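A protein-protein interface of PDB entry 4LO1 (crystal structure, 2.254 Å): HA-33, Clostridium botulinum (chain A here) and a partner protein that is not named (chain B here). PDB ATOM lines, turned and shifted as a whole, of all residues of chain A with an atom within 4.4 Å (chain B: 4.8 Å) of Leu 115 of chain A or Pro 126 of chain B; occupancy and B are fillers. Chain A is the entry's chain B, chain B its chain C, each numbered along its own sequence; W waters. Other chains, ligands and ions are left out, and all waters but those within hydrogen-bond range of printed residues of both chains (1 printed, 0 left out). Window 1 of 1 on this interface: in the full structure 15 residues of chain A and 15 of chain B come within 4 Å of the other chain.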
ATOM      1  N   TRP A  74     -24.722  -6.969 -32.367  1.00  0.00           N
ATOM      2  CA  TRP A  74     -24.668  -6.186 -31.132  1.00  0.00           C
ATOM      3  C   TRP A  74     -25.574  -6.816 -30.084  1.00  0.00           C
ATOM      4  O   TRP A  74     -26.793  -6.881 -30.255  1.00  0.00           O
ATOM      5  CB  TRP A  74     -25.093  -4.734 -31.373  1.00  0.00           C
ATOM      6  CG  TRP A  74     -25.330  -3.939 -30.104  1.00  0.00           C
ATOM      7  CD1 TRP A  74     -24.705  -4.105 -28.898  1.00  0.00           C
ATOM      8  CD2 TRP A  74     -26.268  -2.867 -29.919  1.00  0.00           C
ATOM      9  NE1 TRP A  74     -25.193  -3.207 -27.982  1.00  0.00           N
ATOM     10  CE2 TRP A  74     -26.152  -2.435 -28.582  1.00  0.00           C
ATOM     11  CE3 TRP A  74     -27.192  -2.230 -30.756  1.00  0.00           C
ATOM     12  CZ2 TRP A  74     -26.922  -1.393 -28.062  1.00  0.00           C
ATOM     13  CZ3 TRP A  74     -27.958  -1.196 -30.237  1.00  0.00           C
ATOM     14  CH2 TRP A  74     -27.818  -0.789 -28.901  1.00  0.00           C
ATOM     15  N   PRO A  77     -28.860  -4.905 -24.671  1.00  0.00           N
ATOM     16  CA  PRO A  77     -28.334  -3.545 -24.487  1.00  0.00           C
ATOM     17  C   PRO A  77     -26.888  -3.492 -23.996  1.00  0.00           C
ATOM     18  O   PRO A  77     -26.419  -2.413 -23.624  1.00  0.00           O
ATOM     19  CB  PRO A  77     -29.240  -2.991 -23.394  1.00  0.00           C
ATOM     20  CG  PRO A  77     -29.494  -4.219 -22.512  1.00  0.00           C
ATOM     21  CD  PRO A  77     -29.517  -5.409 -23.446  1.00  0.00           C
ATOM     22  N   ALA A 108     -21.704   2.145 -37.698  1.00  0.00           N
ATOM     23  CA  ALA A 108     -22.756   2.482 -36.747  1.00  0.00           C
ATOM     24  C   ALA A 108     -23.860   1.430 -36.709  1.00  0.00           C
ATOM     25  O   ALA A 108     -24.254   0.896 -37.744  1.00  0.00           O
ATOM     26  CB  ALA A 108     -23.347   3.860 -37.088  1.00  0.00           C
ATOM     27  N   SER A 109     -24.363   1.132 -35.516  1.00  0.00           N
ATOM     28  CA  SER A 109     -25.436   0.153 -35.389  1.00  0.00           C
ATOM     29  C   SER A 109     -26.736   0.666 -35.995  1.00  0.00           C
ATOM     30  O   SER A 109     -27.140   1.795 -35.747  1.00  0.00           O
ATOM     31  CB  SER A 109     -25.677  -0.212 -33.927  1.00  0.00           C
ATOM     32  OG  SER A 109     -26.837  -1.022 -33.811  1.00  0.00           O
ATOM     33  N   ASN A 112     -29.231   1.265 -33.203  1.00  0.00           N
ATOM     34  CA  ASN A 112     -29.034   2.538 -32.516  1.00  0.00           C
ATOM     35  C   ASN A 112     -27.859   3.286 -33.128  1.00  0.00           C
ATOM     36  O   ASN A 112     -26.716   3.105 -32.709  1.00  0.00           O
ATOM     37  CB  ASN A 112     -28.800   2.319 -31.020  1.00  0.00           C
ATOM     38  CG  ASN A 112     -28.874   3.609 -30.217  1.00  0.00           C
ATOM     39  OD1 ASN A 112     -28.591   4.694 -30.725  1.00  0.00           O
ATOM     40  ND2 ASN A 112     -29.252   3.490 -28.951  1.00  0.00           N
ATOM     41  N   PRO A 113     -28.144   4.134 -34.126  1.00  0.00           N
ATOM     42  CA  PRO A 113     -27.147   4.887 -34.898  1.00  0.00           C
ATOM     43  C   PRO A 113     -26.264   5.794 -34.041  1.00  0.00           C
ATOM     44  O   PRO A 113     -25.229   6.252 -34.519  1.00  0.00           O
ATOM     45  CB  PRO A 113     -28.007   5.731 -35.843  1.00  0.00           C
ATOM     46  CG  PRO A 113     -29.289   4.994 -35.955  1.00  0.00           C
ATOM     47  CD  PRO A 113     -29.511   4.359 -34.621  1.00  0.00           C
ATOM     48  N   ASN A 114     -26.667   6.057 -32.802  1.00  0.00           N
ATOM     49  CA  ASN A 114     -25.823   6.810 -31.880  1.00  0.00           C
ATOM     50  C   ASN A 114     -24.591   6.006 -31.498  1.00  0.00           C
ATOM     51  O   ASN A 114     -23.581   6.566 -31.073  1.00  0.00           O
ATOM     52  CB  ASN A 114     -26.581   7.182 -30.603  1.00  0.00           C
ATOM     53  CG  ASN A 114     -27.826   7.997 -30.875  1.00  0.00           C
ATOM     54  OD1 ASN A 114     -28.939   7.567 -30.578  1.00  0.00           O
ATOM     55  ND2 ASN A 114     -27.643   9.187 -31.425  1.00  0.00           N
ATOM     56  N   LEU A 115     -24.686   4.686 -31.637  1.00  0.00           N
ATOM     57  CA  LEU A 115     -23.617   3.792 -31.207  1.00  0.00           C
ATOM     58  C   LEU A 115     -22.847   3.206 -32.382  1.00  0.00           C
ATOM     59  O   LEU A 115     -23.431   2.717 -33.350  1.00  0.00           O
ATOM     60  CB  LEU A 115     -24.184   2.677 -30.328  1.00  0.00           C
ATOM     61  CG  LEU A 115     -24.820   3.159 -29.024  1.00  0.00           C
ATOM     62  CD1 LEU A 115     -25.366   1.990 -28.224  1.00  0.00           C
ATOM     63  CD2 LEU A 115     -23.801   3.938 -28.213  1.00  0.00           C
ATOM     64  N   VAL A 116     -21.524   3.266 -32.291  1.00  0.00           N
ATOM     65  CA  VAL A 116     -20.664   2.775 -33.355  1.00  0.00           C
ATOM     66  C   VAL A 116     -19.634   1.819 -32.770  1.00  0.00           C
ATOM     67  O   VAL A 116     -19.393   1.824 -31.562  1.00  0.00           O
ATOM     68  CB  VAL A 116     -19.942   3.931 -34.083  1.00  0.00           C
ATOM     69  CG1 VAL A 116     -20.943   4.991 -34.513  1.00  0.00           C
ATOM     70  CG2 VAL A 116     -18.881   4.548 -33.191  1.00  0.00           C
ATOM     71  N   LEU A 128     -18.832  -0.757 -28.083  1.00  0.00           N
ATOM     72  CA  LEU A 128     -19.618   0.322 -28.672  1.00  0.00           C
ATOM     73  C   LEU A 128     -19.333   1.684 -28.048  1.00  0.00           C
ATOM     74  O   LEU A 128     -18.874   1.790 -26.911  1.00  0.00           O
ATOM     75  CB  LEU A 128     -21.116   0.010 -28.604  1.00  0.00           C
ATOM     76  CG  LEU A 128     -21.652  -1.088 -29.526  1.00  0.00           C
ATOM     77  CD1 LEU A 128     -23.164  -1.101 -29.483  1.00  0.00           C
ATOM     78  CD2 LEU A 128     -21.164  -0.904 -30.958  1.00  0.00           C
ATOM     79  N   SER A 129     -19.606   2.733 -28.810  1.00  0.00           N
ATOM     80  CA  SER A 129     -19.344   4.086 -28.346  1.00  0.00           C
ATOM     81  C   SER A 129     -20.135   5.091 -29.158  1.00  0.00           C
ATOM     82  O   SER A 129     -20.415   4.867 -30.336  1.00  0.00           O
ATOM     83  CB  SER A 129     -17.854   4.402 -28.467  1.00  0.00           C
ATOM     84  OG  SER A 129     -17.599   5.766 -28.201  1.00  0.00           O
ATOM     85  N   THR A 130     -20.505   6.196 -28.519  1.00  0.00           N
ATOM     86  CA  THR A 130     -21.022   7.343 -29.245  1.00  0.00           C
ATOM     87  C   THR A 130     -19.881   7.936 -30.062  1.00  0.00           C
ATOM     88  O   THR A 130     -18.710   7.655 -29.799  1.00  0.00           O
ATOM     89  CB  THR A 130     -21.599   8.407 -28.295  1.00  0.00           C
ATOM     90  OG1 THR A 130     -20.597   8.804 -27.349  1.00  0.00           O
ATOM     91  CG2 THR A 130     -22.797   7.848 -27.550  1.00  0.00           C
ATOM     92  N   SER B  32     -24.632  -2.316 -18.550  1.00  0.00           N
ATOM     93  CA  SER B  32     -25.501  -1.298 -19.137  1.00  0.00           C
ATOM     94  C   SER B  32     -26.808  -1.145 -18.367  1.00  0.00           C
ATOM     95  O   SER B  32     -27.168  -1.991 -17.549  1.00  0.00           O
ATOM     96  CB  SER B  32     -25.807  -1.618 -20.605  1.00  0.00           C
ATOM     97  OG  SER B  32     -24.618  -1.753 -21.361  1.00  0.00           O
ATOM     98  N   LEU B  33     -27.509  -0.052 -18.641  1.00  0.00           N
ATOM     99  CA  LEU B  33     -28.809   0.218 -18.041  1.00  0.00           C
ATOM    100  C   LEU B  33     -29.864   0.130 -19.130  1.00  0.00           C
ATOM    101  O   LEU B  33     -29.665   0.633 -20.233  1.00  0.00           O
ATOM    102  CB  LEU B  33     -28.839   1.615 -17.409  1.00  0.00           C
ATOM    103  CG  LEU B  33     -28.211   1.834 -16.028  1.00  0.00           C
ATOM    104  CD1 LEU B  33     -28.869   0.935 -14.986  1.00  0.00           C
ATOM    105  CD2 LEU B  33     -26.699   1.630 -16.050  1.00  0.00           C
ATOM    106  N   THR B  34     -30.989  -0.501 -18.825  1.00  0.00           N
ATOM    107  CA  THR B  34     -32.045  -0.652 -19.814  1.00  0.00           C
ATOM    108  C   THR B  34     -33.415  -0.736 -19.152  1.00  0.00           C
ATOM    109  O   THR B  34     -33.519  -0.840 -17.930  1.00  0.00           O
ATOM    110  CB  THR B  34     -31.818  -1.900 -20.687  1.00  0.00           C
ATOM    111  OG1 THR B  34     -32.572  -1.785 -21.899  1.00  0.00           O
ATOM    112  CG2 THR B  34     -32.232  -3.169 -19.936  1.00  0.00           C
ATOM    113  N   PHE B  76     -22.353   5.785 -22.423  1.00  0.00           N
ATOM    114  CA  PHE B  76     -23.333   4.957 -21.726  1.00  0.00           C
ATOM    115  C   PHE B  76     -23.570   5.453 -20.303  1.00  0.00           C
ATOM    116  O   PHE B  76     -22.647   5.917 -19.638  1.00  0.00           O
ATOM    117  CB  PHE B  76     -22.848   3.507 -21.642  1.00  0.00           C
ATOM    118  CG  PHE B  76     -22.952   2.737 -22.930  1.00  0.00           C
ATOM    119  CD1 PHE B  76     -22.048   2.950 -23.956  1.00  0.00           C
ATOM    120  CD2 PHE B  76     -23.930   1.766 -23.093  1.00  0.00           C
ATOM    121  CE1 PHE B  76     -22.131   2.227 -25.132  1.00  0.00           C
ATOM    122  CE2 PHE B  76     -24.019   1.039 -24.270  1.00  0.00           C
ATOM    123  CZ  PHE B  76     -23.116   1.270 -25.289  1.00  0.00           C
ATOM    124  N   ASP B 114     -30.698   9.645 -22.231  1.00  0.00           N
ATOM    125  CA  ASP B 114     -31.347   9.571 -23.528  1.00  0.00           C
ATOM    126  C   ASP B 114     -31.578   8.112 -23.879  1.00  0.00           C
ATOM    127  O   ASP B 114     -30.647   7.307 -23.874  1.00  0.00           O
ATOM    128  CB  ASP B 114     -30.488  10.257 -24.596  1.00  0.00           C
ATOM    129  CG  ASP B 114     -31.246  10.509 -25.894  1.00  0.00           C
ATOM    130  OD1 ASP B 114     -31.846   9.562 -26.449  1.00  0.00           O
ATOM    131  OD2 ASP B 114     -31.239  11.665 -26.362  1.00  0.00           O
ATOM    132  N   ILE B 115     -32.825   7.771 -24.173  1.00  0.00           N
ATOM    133  CA  ILE B 115     -33.144   6.421 -24.608  1.00  0.00           C
ATOM    134  C   ILE B 115     -33.641   6.448 -26.053  1.00  0.00           C
ATOM    135  O   ILE B 115     -34.577   7.178 -26.391  1.00  0.00           O
ATOM    136  CB  ILE B 115     -34.157   5.730 -23.657  1.00  0.00           C
ATOM    137  CG1 ILE B 115     -34.303   4.243 -24.002  1.00  0.00           C
ATOM    138  CG2 ILE B 115     -35.503   6.458 -23.636  1.00  0.00           C
ATOM    139  CD1 ILE B 115     -33.117   3.393 -23.561  1.00  0.00           C
ATOM    140  N   SER B 124     -34.529  -3.446 -25.353  1.00  0.00           N
ATOM    141  CA  SER B 124     -33.116  -3.785 -25.540  1.00  0.00           C
ATOM    142  C   SER B 124     -32.197  -2.582 -25.773  1.00  0.00           C
ATOM    143  O   SER B 124     -31.005  -2.757 -25.998  1.00  0.00           O
ATOM    144  CB  SER B 124     -32.931  -4.823 -26.656  1.00  0.00           C
ATOM    145  OG  SER B 124     -33.747  -5.960 -26.442  1.00  0.00           O
ATOM    146  N   GLN B 125     -32.743  -1.370 -25.714  1.00  0.00           N
ATOM    147  CA  GLN B 125     -31.922  -0.168 -25.865  1.00  0.00           C
ATOM    148  C   GLN B 125     -31.211   0.189 -24.562  1.00  0.00           C
ATOM    149  O   GLN B 125     -31.814   0.146 -23.491  1.00  0.00           O
ATOM    150  CB  GLN B 125     -32.768   1.026 -26.324  1.00  0.00           C
ATOM    151  CG  GLN B 125     -33.343   0.905 -27.726  1.00  0.00           C
ATOM    152  CD  GLN B 125     -32.301   1.092 -28.816  1.00  0.00           C
ATOM    153  OE1 GLN B 125     -31.152   1.438 -28.546  1.00  0.00           O
ATOM    154  NE2 GLN B 125     -32.705   0.867 -30.059  1.00  0.00           N
ATOM    155  N   PRO B 126     -29.920   0.540 -24.649  1.00  0.00           N
ATOM    156  CA  PRO B 126     -29.194   1.019 -23.472  1.00  0.00           C
ATOM    157  C   PRO B 126     -29.479   2.496 -23.235  1.00  0.00           C
ATOM    158  O   PRO B 126     -29.722   3.241 -24.187  1.00  0.00           O
ATOM    159  CB  PRO B 126     -27.731   0.828 -23.869  1.00  0.00           C
ATOM    160  CG  PRO B 126     -27.733   0.995 -25.351  1.00  0.00           C
ATOM    161  CD  PRO B 126     -29.052   0.446 -25.836  1.00  0.00           C
ATOM    162  N   LEU B 127     -29.466   2.909 -21.974  1.00  0.00           N
ATOM    163  CA  LEU B 127     -29.636   4.311 -21.637  1.00  0.00           C
ATOM    164  C   LEU B 127     -28.317   5.027 -21.897  1.00  0.00           C
ATOM    165  O   LEU B 127     -27.269   4.610 -21.399  1.00  0.00           O
ATOM    166  CB  LEU B 127     -30.048   4.454 -20.172  1.00  0.00           C
ATOM    167  CG  LEU B 127     -30.461   5.850 -19.699  1.00  0.00           C
ATOM    168  CD1 LEU B 127     -31.644   6.354 -20.503  1.00  0.00           C
ATOM    169  CD2 LEU B 127     -30.784   5.835 -18.208  1.00  0.00           C
ATOM    170  N   LEU B 128     -28.364   6.091 -22.692  1.00  0.00           N
ATOM    171  CA  LEU B 128     -27.154   6.823 -23.051  1.00  0.00           C
ATOM    172  C   LEU B 128     -27.116   8.229 -22.451  1.00  0.00           C
ATOM    173  O   LEU B 128     -28.109   8.714 -21.901  1.00  0.00           O
ATOM    174  CB  LEU B 128     -27.016   6.902 -24.573  1.00  0.00           C
ATOM    175  CG  LEU B 128     -27.070   5.582 -25.348  1.00  0.00           C
ATOM    176  CD1 LEU B 128     -26.920   5.840 -26.842  1.00  0.00           C
ATOM    177  CD2 LEU B 128     -26.005   4.612 -24.855  1.00  0.00           C
HETATM  178  O   HOH W   1     -30.736   4.650 -26.361  1.00  0.00           O
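The side-chain amide nitrogen (ND2) of Asn 112 of chain A lies within hydrogen-bond range of the side-chain amide oxygen (OE1) of Gln 125 of chain B, at 2.8 Å. The side-chain hydroxyl (OG) of Ser 32 of chain B is in hydrogen-bond range of the backbone carbonyl oxygen (O) of Pro 77 of chain A (3.0 Å). N of Pro 77 of chain A sits close to O of Ser 124 of chain B (3.3 Å).
OD1 of Asn 112 of chain A lies close to OD1 of Asn 114 of chain A (2.9 Å). OG1 of Thr 34 of chain B is in hydrogen-bond range of O of Gln 125 of chain B, 2.6 Å away. N of Asp 114 of chain B is in hydrogen-bond range of O of Leu 128 of chain B (2.8 Å). The backbone carbonyl oxygen of Leu 115 of chain A sits at hydrogen-bond distance from the backbone NH of Ser 109 of chain A. The side-chain hydroxyl of Ser 109 of chain A lies within hydrogen-bond range of the backbone NH of Asn 112 of chain A (3.4 Å).
Trp 74 of chain A touches Pro 126 of chain B. CG of Pro 77 of chain A touches CB of Thr 34 of chain B (3.8 Å). Pro 77 of chain A touches Gln 125 of chain B. Pro 126 of chain B touches Pro 77 of chain A. Asn 112 of chain A touches Leu 128 of chain B (ND2 to CD1, 3.9 Å). Leu 115 of chain A touches Phe 76 of chain B (CD1 to CZ, 3.8 Å). Leu 115 of chain A touches Pro 126 of chain B. Leu 115 of chain A touches Leu 128 of chain B (CD2 to CD1, 3.9 Å). Phe 76 of chain B touches Leu 128 of chain A.
Of the printed residues of chain B, Trp 74 of chain A touches Pro 126 (3.5 Å). Printed residues of chain B within 4 Å of Asn 112 of chain A: Gln 125 (2.8 Å) and Leu 128 (3.9 Å). Leu 115 of chain A touches three residues of chain B. Of the printed residues of chain A, Ser 32 of chain B touches Pro 77 (3.0 Å). Leu 33 of chain B touches none of the printed residues of chain A. Of the printed residues of chain A, Phe 76 of chain B touches Leu 115 and Leu 128. Asp 114 of chain B touches none of the printed residues of chain A. Pro 126 of chain B touches just these residues of chain A: Trp 74, Pro 77 and Leu 115. Printed residues of chain A within 4 Å of Leu 128 of chain B: Asn 112 and Leu 115. The nearest printed residue of chain B that does not touch Leu 115 of chain A is Gln 125 of chain B (5.8 Å). The nearest printed residue of chain A that does not touch Pro 126 of chain B is Asn 112 of chain A (4.4 Å). The nearest printed residue of chain B that does not touch Leu 128 of chain A is Pro 126 of chain B (6.5 Å).
Of the 12 printed residues of chain A, 5 touch a printed residue of chain B. Hydrophobic or aromatic side chains of chain A that line the printed part of chain B: Trp 74, Pro 77 and Leu 115. Of the 11 printed residues of chain B, 7 touch a printed residue of chain A. Printed residues of chain B that touch a printed residue of chain A: Ser 32, Thr 34, Phe 76, Ser 124, Gln 125, Pro 126 and Leu 128. Hydrophobic or aromatic side chains of chain B that line the printed part of chain A: Phe 76, Pro 126 and Leu 128.
Water W1 bridges the backbone carbonyl oxygen of Pro 126 of chain B (2.8 Å) and the side-chain amide nitrogen of Asn 112 of chain A (3.2 Å).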
